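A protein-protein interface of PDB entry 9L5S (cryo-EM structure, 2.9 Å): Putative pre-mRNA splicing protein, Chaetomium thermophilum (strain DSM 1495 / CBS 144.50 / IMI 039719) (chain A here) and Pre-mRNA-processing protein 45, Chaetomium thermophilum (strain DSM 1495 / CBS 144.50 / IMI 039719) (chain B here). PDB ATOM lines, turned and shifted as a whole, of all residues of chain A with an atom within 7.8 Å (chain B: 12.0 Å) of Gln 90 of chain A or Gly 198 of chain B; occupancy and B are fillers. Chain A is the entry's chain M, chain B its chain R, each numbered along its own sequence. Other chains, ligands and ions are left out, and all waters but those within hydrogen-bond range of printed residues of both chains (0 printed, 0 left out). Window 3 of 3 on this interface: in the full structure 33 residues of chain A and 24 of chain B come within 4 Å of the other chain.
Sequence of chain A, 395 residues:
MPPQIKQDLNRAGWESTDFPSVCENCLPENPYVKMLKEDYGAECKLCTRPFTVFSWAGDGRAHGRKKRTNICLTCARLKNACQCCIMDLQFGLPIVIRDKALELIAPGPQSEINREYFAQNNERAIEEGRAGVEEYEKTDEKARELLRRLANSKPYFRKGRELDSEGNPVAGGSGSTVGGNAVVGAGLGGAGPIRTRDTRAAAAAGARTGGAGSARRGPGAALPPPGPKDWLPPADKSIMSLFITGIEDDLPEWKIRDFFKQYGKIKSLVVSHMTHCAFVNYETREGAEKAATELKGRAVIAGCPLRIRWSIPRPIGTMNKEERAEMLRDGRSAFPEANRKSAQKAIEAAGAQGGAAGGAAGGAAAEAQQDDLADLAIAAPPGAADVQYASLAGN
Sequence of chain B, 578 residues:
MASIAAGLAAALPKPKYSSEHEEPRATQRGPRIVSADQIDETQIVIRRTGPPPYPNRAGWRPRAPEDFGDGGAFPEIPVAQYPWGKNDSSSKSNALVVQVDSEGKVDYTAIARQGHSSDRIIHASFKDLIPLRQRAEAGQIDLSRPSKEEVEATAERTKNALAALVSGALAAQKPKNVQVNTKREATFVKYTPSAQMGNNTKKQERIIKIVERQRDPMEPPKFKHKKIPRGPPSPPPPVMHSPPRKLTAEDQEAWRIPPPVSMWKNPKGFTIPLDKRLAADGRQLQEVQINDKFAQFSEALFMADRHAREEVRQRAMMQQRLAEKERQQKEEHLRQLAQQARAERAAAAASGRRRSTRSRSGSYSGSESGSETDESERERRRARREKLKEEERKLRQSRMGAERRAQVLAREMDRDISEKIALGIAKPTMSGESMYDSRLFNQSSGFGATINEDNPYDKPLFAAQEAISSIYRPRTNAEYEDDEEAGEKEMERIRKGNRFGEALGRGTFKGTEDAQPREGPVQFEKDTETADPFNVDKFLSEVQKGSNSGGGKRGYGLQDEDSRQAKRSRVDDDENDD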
ATOM      1  N   ASN A  80     -19.904  -6.730 -17.129  1.00  0.00           N
ATOM      2  CA  ASN A  80     -19.338  -5.389 -17.314  1.00  0.00           C
ATOM      3  C   ASN A  80     -20.317  -4.313 -16.844  1.00  0.00           C
ATOM      4  O   ASN A  80     -20.761  -3.454 -17.607  1.00  0.00           O
ATOM      5  CB  ASN A  80     -18.911  -5.157 -18.765  1.00  0.00           C
ATOM      6  CG  ASN A  80     -17.761  -4.179 -18.881  1.00  0.00           C
ATOM      7  OD1 ASN A  80     -16.892  -4.119 -18.012  1.00  0.00           O
ATOM      8  ND2 ASN A  80     -17.749  -3.403 -19.959  1.00  0.00           N
ATOM      9  N   ALA A  81     -20.651  -4.379 -15.558  1.00  0.00           N
ATOM     10  CA  ALA A  81     -21.702  -3.545 -15.000  1.00  0.00           C
ATOM     11  C   ALA A  81     -21.297  -3.033 -13.627  1.00  0.00           C
ATOM     12  O   ALA A  81     -20.459  -3.624 -12.941  1.00  0.00           O
ATOM     13  CB  ALA A  81     -23.028  -4.309 -14.903  1.00  0.00           C
ATOM     14  N   CYS A  82     -21.902  -1.911 -13.241  1.00  0.00           N
ATOM     15  CA  CYS A  82     -21.761  -1.410 -11.882  1.00  0.00           C
ATOM     16  C   CYS A  82     -22.412  -2.373 -10.901  1.00  0.00           C
ATOM     17  O   CYS A  82     -23.440  -2.990 -11.197  1.00  0.00           O
ATOM     18  CB  CYS A  82     -22.390  -0.024 -11.745  1.00  0.00           C
ATOM     19  SG  CYS A  82     -22.494   0.590 -10.037  1.00  0.00           S
ATOM     20  N   MET A  87     -26.091  -1.632 -14.535  1.00  0.00           N
ATOM     21  CA  MET A  87     -26.171  -1.152 -15.905  1.00  0.00           C
ATOM     22  C   MET A  87     -24.788  -1.208 -16.537  1.00  0.00           C
ATOM     23  O   MET A  87     -23.772  -1.212 -15.840  1.00  0.00           O
ATOM     24  CB  MET A  87     -26.726   0.280 -16.022  1.00  0.00           C
ATOM     25  CG  MET A  87     -27.825   0.653 -15.049  1.00  0.00           C
ATOM     26  SD  MET A  87     -28.399   2.347 -15.309  1.00  0.00           S
ATOM     27  CE  MET A  87     -27.166   3.315 -14.446  1.00  0.00           C
ATOM     28  N   ASP A  88     -24.772  -1.260 -17.872  1.00  0.00           N
ATOM     29  CA  ASP A  88     -23.528  -1.301 -18.637  1.00  0.00           C
ATOM     30  C   ASP A  88     -22.638  -0.102 -18.330  1.00  0.00           C
ATOM     31  O   ASP A  88     -23.100   1.042 -18.305  1.00  0.00           O
ATOM     32  CB  ASP A  88     -23.840  -1.349 -20.132  1.00  0.00           C
ATOM     33  CG  ASP A  88     -22.592  -1.429 -20.983  1.00  0.00           C
ATOM     34  OD1 ASP A  88     -21.956  -2.501 -21.018  1.00  0.00           O
ATOM     35  OD2 ASP A  88     -22.246  -0.414 -21.620  1.00  0.00           O
ATOM     36  N   LEU A  89     -21.356  -0.373 -18.088  1.00  0.00           N
ATOM     37  CA  LEU A  89     -20.396   0.653 -17.707  1.00  0.00           C
ATOM     38  C   LEU A  89     -19.708   1.300 -18.903  1.00  0.00           C
ATOM     39  O   LEU A  89     -18.668   1.946 -18.732  1.00  0.00           O
ATOM     40  CB  LEU A  89     -19.356   0.075 -16.746  1.00  0.00           C
ATOM     41  CG  LEU A  89     -19.766   0.195 -15.275  1.00  0.00           C
ATOM     42  CD1 LEU A  89     -18.664  -0.268 -14.347  1.00  0.00           C
ATOM     43  CD2 LEU A  89     -20.161   1.624 -14.956  1.00  0.00           C
ATOM     44  N   GLN A  90     -20.253   1.135 -20.103  1.00  0.00           N
ATOM     45  CA  GLN A  90     -19.761   1.840 -21.277  1.00  0.00           C
ATOM     46  C   GLN A  90     -20.790   2.765 -21.907  1.00  0.00           C
ATOM     47  O   GLN A  90     -20.410   3.811 -22.437  1.00  0.00           O
ATOM     48  CB  GLN A  90     -19.268   0.846 -22.340  1.00  0.00           C
ATOM     49  CG  GLN A  90     -18.153  -0.069 -21.865  1.00  0.00           C
ATOM     50  CD  GLN A  90     -17.570  -0.907 -22.985  1.00  0.00           C
ATOM     51  OE1 GLN A  90     -17.961  -0.770 -24.145  1.00  0.00           O
ATOM     52  NE2 GLN A  90     -16.626  -1.776 -22.646  1.00  0.00           N
ATOM     53  N   PHE A  91     -22.076   2.415 -21.863  1.00  0.00           N
ATOM     54  CA  PHE A  91     -23.127   3.250 -22.422  1.00  0.00           C
ATOM     55  C   PHE A  91     -24.205   3.635 -21.421  1.00  0.00           C
ATOM     56  O   PHE A  91     -25.043   4.483 -21.744  1.00  0.00           O
ATOM     57  CB  PHE A  91     -23.788   2.549 -23.619  1.00  0.00           C
ATOM     58  CG  PHE A  91     -22.808   1.995 -24.610  1.00  0.00           C
ATOM     59  CD1 PHE A  91     -22.112   2.838 -25.461  1.00  0.00           C
ATOM     60  CD2 PHE A  91     -22.580   0.631 -24.690  1.00  0.00           C
ATOM     61  CE1 PHE A  91     -21.206   2.331 -26.373  1.00  0.00           C
ATOM     62  CE2 PHE A  91     -21.676   0.116 -25.601  1.00  0.00           C
ATOM     63  CZ  PHE A  91     -20.988   0.969 -26.443  1.00  0.00           C
ATOM     64  N   GLY A  92     -24.207   3.056 -20.226  1.00  0.00           N
ATOM     65  CA  GLY A  92     -25.267   3.324 -19.271  1.00  0.00           C
ATOM     66  C   GLY A  92     -26.586   2.680 -19.634  1.00  0.00           C
ATOM     67  O   GLY A  92     -27.646   3.284 -19.425  1.00  0.00           O
ATOM     68  N   LEU A  93     -26.547   1.465 -20.170  1.00  0.00           N
ATOM     69  CA  LEU A  93     -27.711   0.698 -20.576  1.00  0.00           C
ATOM     70  C   LEU A  93     -27.908  -0.499 -19.654  1.00  0.00           C
ATOM     71  O   LEU A  93     -26.943  -0.992 -19.064  1.00  0.00           O
ATOM     72  CB  LEU A  93     -27.563   0.187 -22.014  1.00  0.00           C
ATOM     73  CG  LEU A  93     -27.787   1.174 -23.154  1.00  0.00           C
ATOM     74  CD1 LEU A  93     -27.002   0.733 -24.376  1.00  0.00           C
ATOM     75  CD2 LEU A  93     -29.266   1.298 -23.479  1.00  0.00           C
ATOM     76  N   ARG A  98     -28.558  -4.053 -23.629  1.00  0.00           N
ATOM     77  CA  ARG A  98     -27.276  -4.054 -24.327  1.00  0.00           C
ATOM     78  C   ARG A  98     -27.048  -5.371 -25.060  1.00  0.00           C
ATOM     79  O   ARG A  98     -26.600  -5.378 -26.213  1.00  0.00           O
ATOM     80  CB  ARG A  98     -26.160  -3.785 -23.309  1.00  0.00           C
ATOM     81  CG  ARG A  98     -24.765  -3.475 -23.852  1.00  0.00           C
ATOM     82  CD  ARG A  98     -23.925  -4.734 -23.989  1.00  0.00           C
ATOM     83  NE  ARG A  98     -23.956  -5.565 -22.791  1.00  0.00           N
ATOM     84  CZ  ARG A  98     -23.087  -5.488 -21.793  1.00  0.00           C
ATOM     85  NH1 ARG A  98     -22.056  -4.663 -21.837  1.00  0.00           N
ATOM     86  NH2 ARG A  98     -23.247  -6.273 -20.732  1.00  0.00           N
ATOM     87  N   LEU A 102     -26.982  -5.572 -29.102  1.00  0.00           N
ATOM     88  CA  LEU A 102     -25.639  -5.719 -29.644  1.00  0.00           C
ATOM     89  C   LEU A 102     -25.263  -7.164 -29.937  1.00  0.00           C
ATOM     90  O   LEU A 102     -24.165  -7.397 -30.459  1.00  0.00           O
ATOM     91  CB  LEU A 102     -24.593  -5.103 -28.702  1.00  0.00           C
ATOM     92  CG  LEU A 102     -24.369  -3.583 -28.699  1.00  0.00           C
ATOM     93  CD1 LEU A 102     -25.510  -2.803 -28.057  1.00  0.00           C
ATOM     94  CD2 LEU A 102     -23.040  -3.246 -28.032  1.00  0.00           C
ATOM     95  N   LEU A 104     -24.525  -9.925 -27.976  1.00  0.00           N
ATOM     96  CA  LEU A 104     -23.317 -10.346 -27.285  1.00  0.00           C
ATOM     97  C   LEU A 104     -23.457 -11.756 -26.725  1.00  0.00           C
ATOM     98  O   LEU A 104     -24.557 -12.302 -26.606  1.00  0.00           O
ATOM     99  CB  LEU A 104     -22.943  -9.376 -26.165  1.00  0.00           C
ATOM    100  CG  LEU A 104     -22.197  -8.124 -26.630  1.00  0.00           C
ATOM    101  CD1 LEU A 104     -21.801  -7.272 -25.446  1.00  0.00           C
ATOM    102  CD2 LEU A 104     -20.974  -8.493 -27.453  1.00  0.00           C
ATOM    103  N   LYS A 138     -15.220  -5.683 -24.883  1.00  0.00           N
ATOM    104  CA  LYS A 138     -14.699  -4.858 -25.967  1.00  0.00           C
ATOM    105  C   LYS A 138     -15.661  -4.851 -27.148  1.00  0.00           C
ATOM    106  O   LYS A 138     -15.406  -5.498 -28.164  1.00  0.00           O
ATOM    107  CB  LYS A 138     -13.329  -5.366 -26.423  1.00  0.00           C
ATOM    108  CG  LYS A 138     -12.269  -5.387 -25.336  1.00  0.00           C
ATOM    109  CD  LYS A 138     -10.919  -5.778 -25.911  1.00  0.00           C
ATOM    110  CE  LYS A 138     -10.905  -7.236 -26.341  1.00  0.00           C
ATOM    111  NZ  LYS A 138     -11.096  -8.164 -25.195  1.00  0.00           N
ATOM    112  N   THR A 139     -16.767  -4.116 -27.020  1.00  0.00           N
ATOM    113  CA  THR A 139     -17.771  -4.113 -28.085  1.00  0.00           C
ATOM    114  C   THR A 139     -17.362  -3.170 -29.213  1.00  0.00           C
ATOM    115  O   THR A 139     -17.063  -3.617 -30.326  1.00  0.00           O
ATOM    116  CB  THR A 139     -19.137  -3.719 -27.515  1.00  0.00           C
ATOM    117  OG1 THR A 139     -19.153  -2.313 -27.241  1.00  0.00           O
ATOM    118  CG2 THR A 139     -19.412  -4.479 -26.229  1.00  0.00           C
ATOM    119  N   ASP A 140     -17.296  -1.867 -28.912  1.00  0.00           N
ATOM    120  CA  ASP A 140     -16.862  -0.796 -29.810  1.00  0.00           C
ATOM    121  C   ASP A 140     -17.455  -0.860 -31.216  1.00  0.00           C
ATOM    122  O   ASP A 140     -18.355  -0.084 -31.555  1.00  0.00           O
ATOM    123  CB  ASP A 140     -15.334  -0.786 -29.903  1.00  0.00           C
ATOM    124  CG  ASP A 140     -14.692   0.075 -28.832  1.00  0.00           C
ATOM    125  OD1 ASP A 140     -15.339   1.043 -28.380  1.00  0.00           O
ATOM    126  OD2 ASP A 140     -13.542  -0.215 -28.441  1.00  0.00           O
ATOM    127  N   ALA A 143     -21.291  -1.461 -31.768  1.00  0.00           N
ATOM    128  CA  ALA A 143     -22.133  -0.277 -31.628  1.00  0.00           C
ATOM    129  C   ALA A 143     -22.264   0.461 -32.957  1.00  0.00           C
ATOM    130  O   ALA A 143     -23.359   0.900 -33.333  1.00  0.00           O
ATOM    131  CB  ALA A 143     -21.561   0.645 -30.552  1.00  0.00           C
ATOM    132  N   SER B 194     -12.418   6.546 -13.671  1.00  0.00           N
ATOM    133  CA  SER B 194     -12.260   6.603 -15.115  1.00  0.00           C
ATOM    134  C   SER B 194     -13.543   7.155 -15.734  1.00  0.00           C
ATOM    135  O   SER B 194     -14.426   7.662 -15.037  1.00  0.00           O
ATOM    136  CB  SER B 194     -11.898   5.226 -15.667  1.00  0.00           C
ATOM    137  OG  SER B 194     -11.473   5.313 -17.016  1.00  0.00           O
ATOM    138  N   ALA B 195     -13.660   7.063 -17.054  1.00  0.00           N
ATOM    139  CA  ALA B 195     -14.844   7.521 -17.769  1.00  0.00           C
ATOM    140  C   ALA B 195     -15.768   6.340 -18.027  1.00  0.00           C
ATOM    141  O   ALA B 195     -15.313   5.273 -18.452  1.00  0.00           O
ATOM    142  CB  ALA B 195     -14.459   8.196 -19.086  1.00  0.00           C
ATOM    143  N   GLN B 196     -17.059   6.530 -17.768  1.00  0.00           N
ATOM    144  CA  GLN B 196     -18.025   5.452 -17.923  1.00  0.00           C
ATOM    145  C   GLN B 196     -19.424   6.028 -18.095  1.00  0.00           C
ATOM    146  O   GLN B 196     -19.692   7.180 -17.744  1.00  0.00           O
ATOM    147  CB  GLN B 196     -17.979   4.484 -16.735  1.00  0.00           C
ATOM    148  CG  GLN B 196     -18.515   5.058 -15.441  1.00  0.00           C
ATOM    149  CD  GLN B 196     -17.414   5.376 -14.446  1.00  0.00           C
ATOM    150  OE1 GLN B 196     -16.228   5.332 -14.772  1.00  0.00           O
ATOM    151  NE2 GLN B 196     -17.806   5.705 -13.224  1.00  0.00           N
ATOM    152  N   MET B 197     -20.305   5.188 -18.639  1.00  0.00           N
ATOM    153  CA  MET B 197     -21.704   5.500 -18.951  1.00  0.00           C
ATOM    154  C   MET B 197     -21.822   6.725 -19.861  1.00  0.00           C
ATOM    155  O   MET B 197     -22.477   7.718 -19.533  1.00  0.00           O
ATOM    156  CB  MET B 197     -22.536   5.722 -17.687  1.00  0.00           C
ATOM    157  CG  MET B 197     -22.745   4.534 -16.781  1.00  0.00           C
ATOM    158  SD  MET B 197     -23.819   5.119 -15.451  1.00  0.00           S
ATOM    159  CE  MET B 197     -22.694   6.125 -14.479  1.00  0.00           C
ATOM    160  N   GLY B 198     -21.189   6.644 -21.030  1.00  0.00           N
ATOM    161  CA  GLY B 198     -21.349   7.730 -21.979  1.00  0.00           C
ATOM    162  C   GLY B 198     -20.321   8.822 -21.794  1.00  0.00           C
ATOM    163  O   GLY B 198     -19.264   8.811 -22.433  1.00  0.00           O
ATOM    164  N   ASN B 199     -20.656   9.776 -20.921  1.00  0.00           N
ATOM    165  CA  ASN B 199     -19.897  11.006 -20.733  1.00  0.00           C
ATOM    166  C   ASN B 199     -18.447  10.727 -20.346  1.00  0.00           C
ATOM    167  O   ASN B 199     -18.135   9.746 -19.667  1.00  0.00           O
ATOM    168  CB  ASN B 199     -20.558  11.857 -19.647  1.00  0.00           C
ATOM    169  CG  ASN B 199     -20.940  11.039 -18.426  1.00  0.00           C
ATOM    170  OD1 ASN B 199     -20.875   9.812 -18.448  1.00  0.00           O
ATOM    171  ND2 ASN B 199     -21.344  11.715 -17.357  1.00  0.00           N
ATOM    172  N   ASN B 200     -17.554  11.618 -20.786  1.00  0.00           N
ATOM    173  CA  ASN B 200     -16.117  11.410 -20.659  1.00  0.00           C
ATOM    174  C   ASN B 200     -15.434  12.547 -19.909  1.00  0.00           C
ATOM    175  O   ASN B 200     -14.217  12.718 -20.027  1.00  0.00           O
ATOM    176  CB  ASN B 200     -15.487  11.233 -22.041  1.00  0.00           C
ATOM    177  CG  ASN B 200     -15.996   9.999 -22.757  1.00  0.00           C
ATOM    178  OD1 ASN B 200     -16.658  10.096 -23.791  1.00  0.00           O
ATOM    179  ND2 ASN B 200     -15.700   8.829 -22.205  1.00  0.00           N
ATOM    180  N   THR B 201     -16.193  13.330 -19.148  1.00  0.00           N
ATOM    181  CA  THR B 201     -15.610  14.397 -18.348  1.00  0.00           C
ATOM    182  C   THR B 201     -14.792  13.815 -17.202  1.00  0.00           C
ATOM    183  O   THR B 201     -15.172  12.812 -16.592  1.00  0.00           O
ATOM    184  CB  THR B 201     -16.707  15.305 -17.793  1.00  0.00           C
ATOM    185  OG1 THR B 201     -17.279  14.701 -16.627  1.00  0.00           O
ATOM    186  CG2 THR B 201     -17.797  15.519 -18.834  1.00  0.00           C
ATOM    187  N   LYS B 202     -13.658  14.449 -16.915  1.00  0.00           N
ATOM    188  CA  LYS B 202     -12.793  13.981 -15.840  1.00  0.00           C
ATOM    189  C   LYS B 202     -13.414  14.325 -14.493  1.00  0.00           C
ATOM    190  O   LYS B 202     -13.447  15.494 -14.094  1.00  0.00           O
ATOM    191  CB  LYS B 202     -11.403  14.601 -15.968  1.00  0.00           C
ATOM    192  CG  LYS B 202     -10.477  14.295 -14.800  1.00  0.00           C
ATOM    193  CD  LYS B 202      -9.111  14.929 -14.994  1.00  0.00           C
ATOM    194  CE  LYS B 202      -8.331  14.969 -13.689  1.00  0.00           C
ATOM    195  NZ  LYS B 202      -7.968  13.601 -13.226  1.00  0.00           N
ATOM    196  N   LYS B 203     -13.919  13.310 -13.799  1.00  0.00           N
ATOM    197  CA  LYS B 203     -14.473  13.511 -12.472  1.00  0.00           C
ATOM    198  C   LYS B 203     -13.352  13.693 -11.457  1.00  0.00           C
ATOM    199  O   LYS B 203     -12.231  13.211 -11.646  1.00  0.00           O
ATOM    200  CB  LYS B 203     -15.359  12.331 -12.074  1.00  0.00           C
ATOM    201  CG  LYS B 203     -16.566  12.133 -12.977  1.00  0.00           C
ATOM    202  CD  LYS B 203     -17.452  13.367 -12.993  1.00  0.00           C
ATOM    203  CE  LYS B 203     -18.720  13.126 -13.795  1.00  0.00           C
ATOM    204  NZ  LYS B 203     -19.227  11.736 -13.629  1.00  0.00           N
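Of the 10 printed residues of chain B, 3 touch a printed residue of chain A.
Printed residues of chain B that touch a printed residue of chain A: Gln 196, Met 197 and Gly 198.
OD2 of Asp 88 of chain A is in hydrogen-bond range of N of Phe 91 of chain A (2.8 Å).
The backbone carbonyl oxygen of Leu 93 of chain A is in hydrogen-bond range of the backbone NH of Asp 88 of chain A (2.5 Å).
The side-chain amide oxygen (OE1) of Gln 196 of chain B lies close to the backbone carbonyl oxygen (O) of Ser 194 of chain B (3.0 Å).
The side-chain amide oxygen (OD1) of Asn 199 of chain B lies close to the backbone carbonyl oxygen (O) of Gln 196 of chain B (3.0 Å).
OD1 of Asn 199 of chain B sits close to O of Met 197 of chain B, at 2.9 Å.
The backbone carbonyl oxygen of Gly 198 of chain B sits close to the side-chain amide oxygen of Asn 200 of chain B, at 3.2 Å.
The backbone carbonyl oxygen of Gln 90 of chain A lies within hydrogen-bond range of the backbone NH of Gly 198 of chain B, 3.3 Å away.
Of the printed residues of chain B, Gln 90 of chain A touches Gly 198 (3.3 Å).
Of chain A, only Gln 90 comes within 4 Å of Gly 198 of chain B.
Of the printed residues of chain B, Leu 89 of chain A touches Gln 196 (3.3 Å) and Met 197 (3.6 Å).
Of chain B, only Met 197 comes within 4 Å of Phe 91 of chain A.
Of chain B, only Met 197 (3.7 Å) comes within 4 Å of Gly 92 of chain A.
No residue of chain B comes within 4 Å of Asp 140 of chain A.
Of the printed residues of chain B, Met 87 of chain A touches Met 197.
Of the printed residues of chain A, Gln 196 of chain B touches Leu 89.
Printed residues of chain A within 4 Å of Met 197 of chain B: Met 87 (3.9 Å), Asp 88 (3.8 Å), Leu 89 (3.6 Å), Phe 91 (3.98 Å) and Gly 92 (3.7 Å).
Leu 93 of chain A touches none of the printed residues of chain B.
Arg 98 of chain A touches none of the printed residues of chain B.
The nearest residue of chain B that does not touch Gln 90 of chain A is Met 197 of chain B (4.04 Å).
CE of Met 87 of chain A touches SD of Met 197 of chain B, 3.9 Å away.
Met 197 of chain B touches Asp 88 of chain A (CG to O, 3.8 Å).
Leu 89 of chain A touches Gln 196 of chain B (O to CB, 3.3 Å).
Leu 89 of chain A touches Met 197 of chain B.
Met 197 of chain B touches Phe 91 of chain A.
Met 197 of chain B touches Gly 92 of chain A (CA to N, 3.7 Å).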
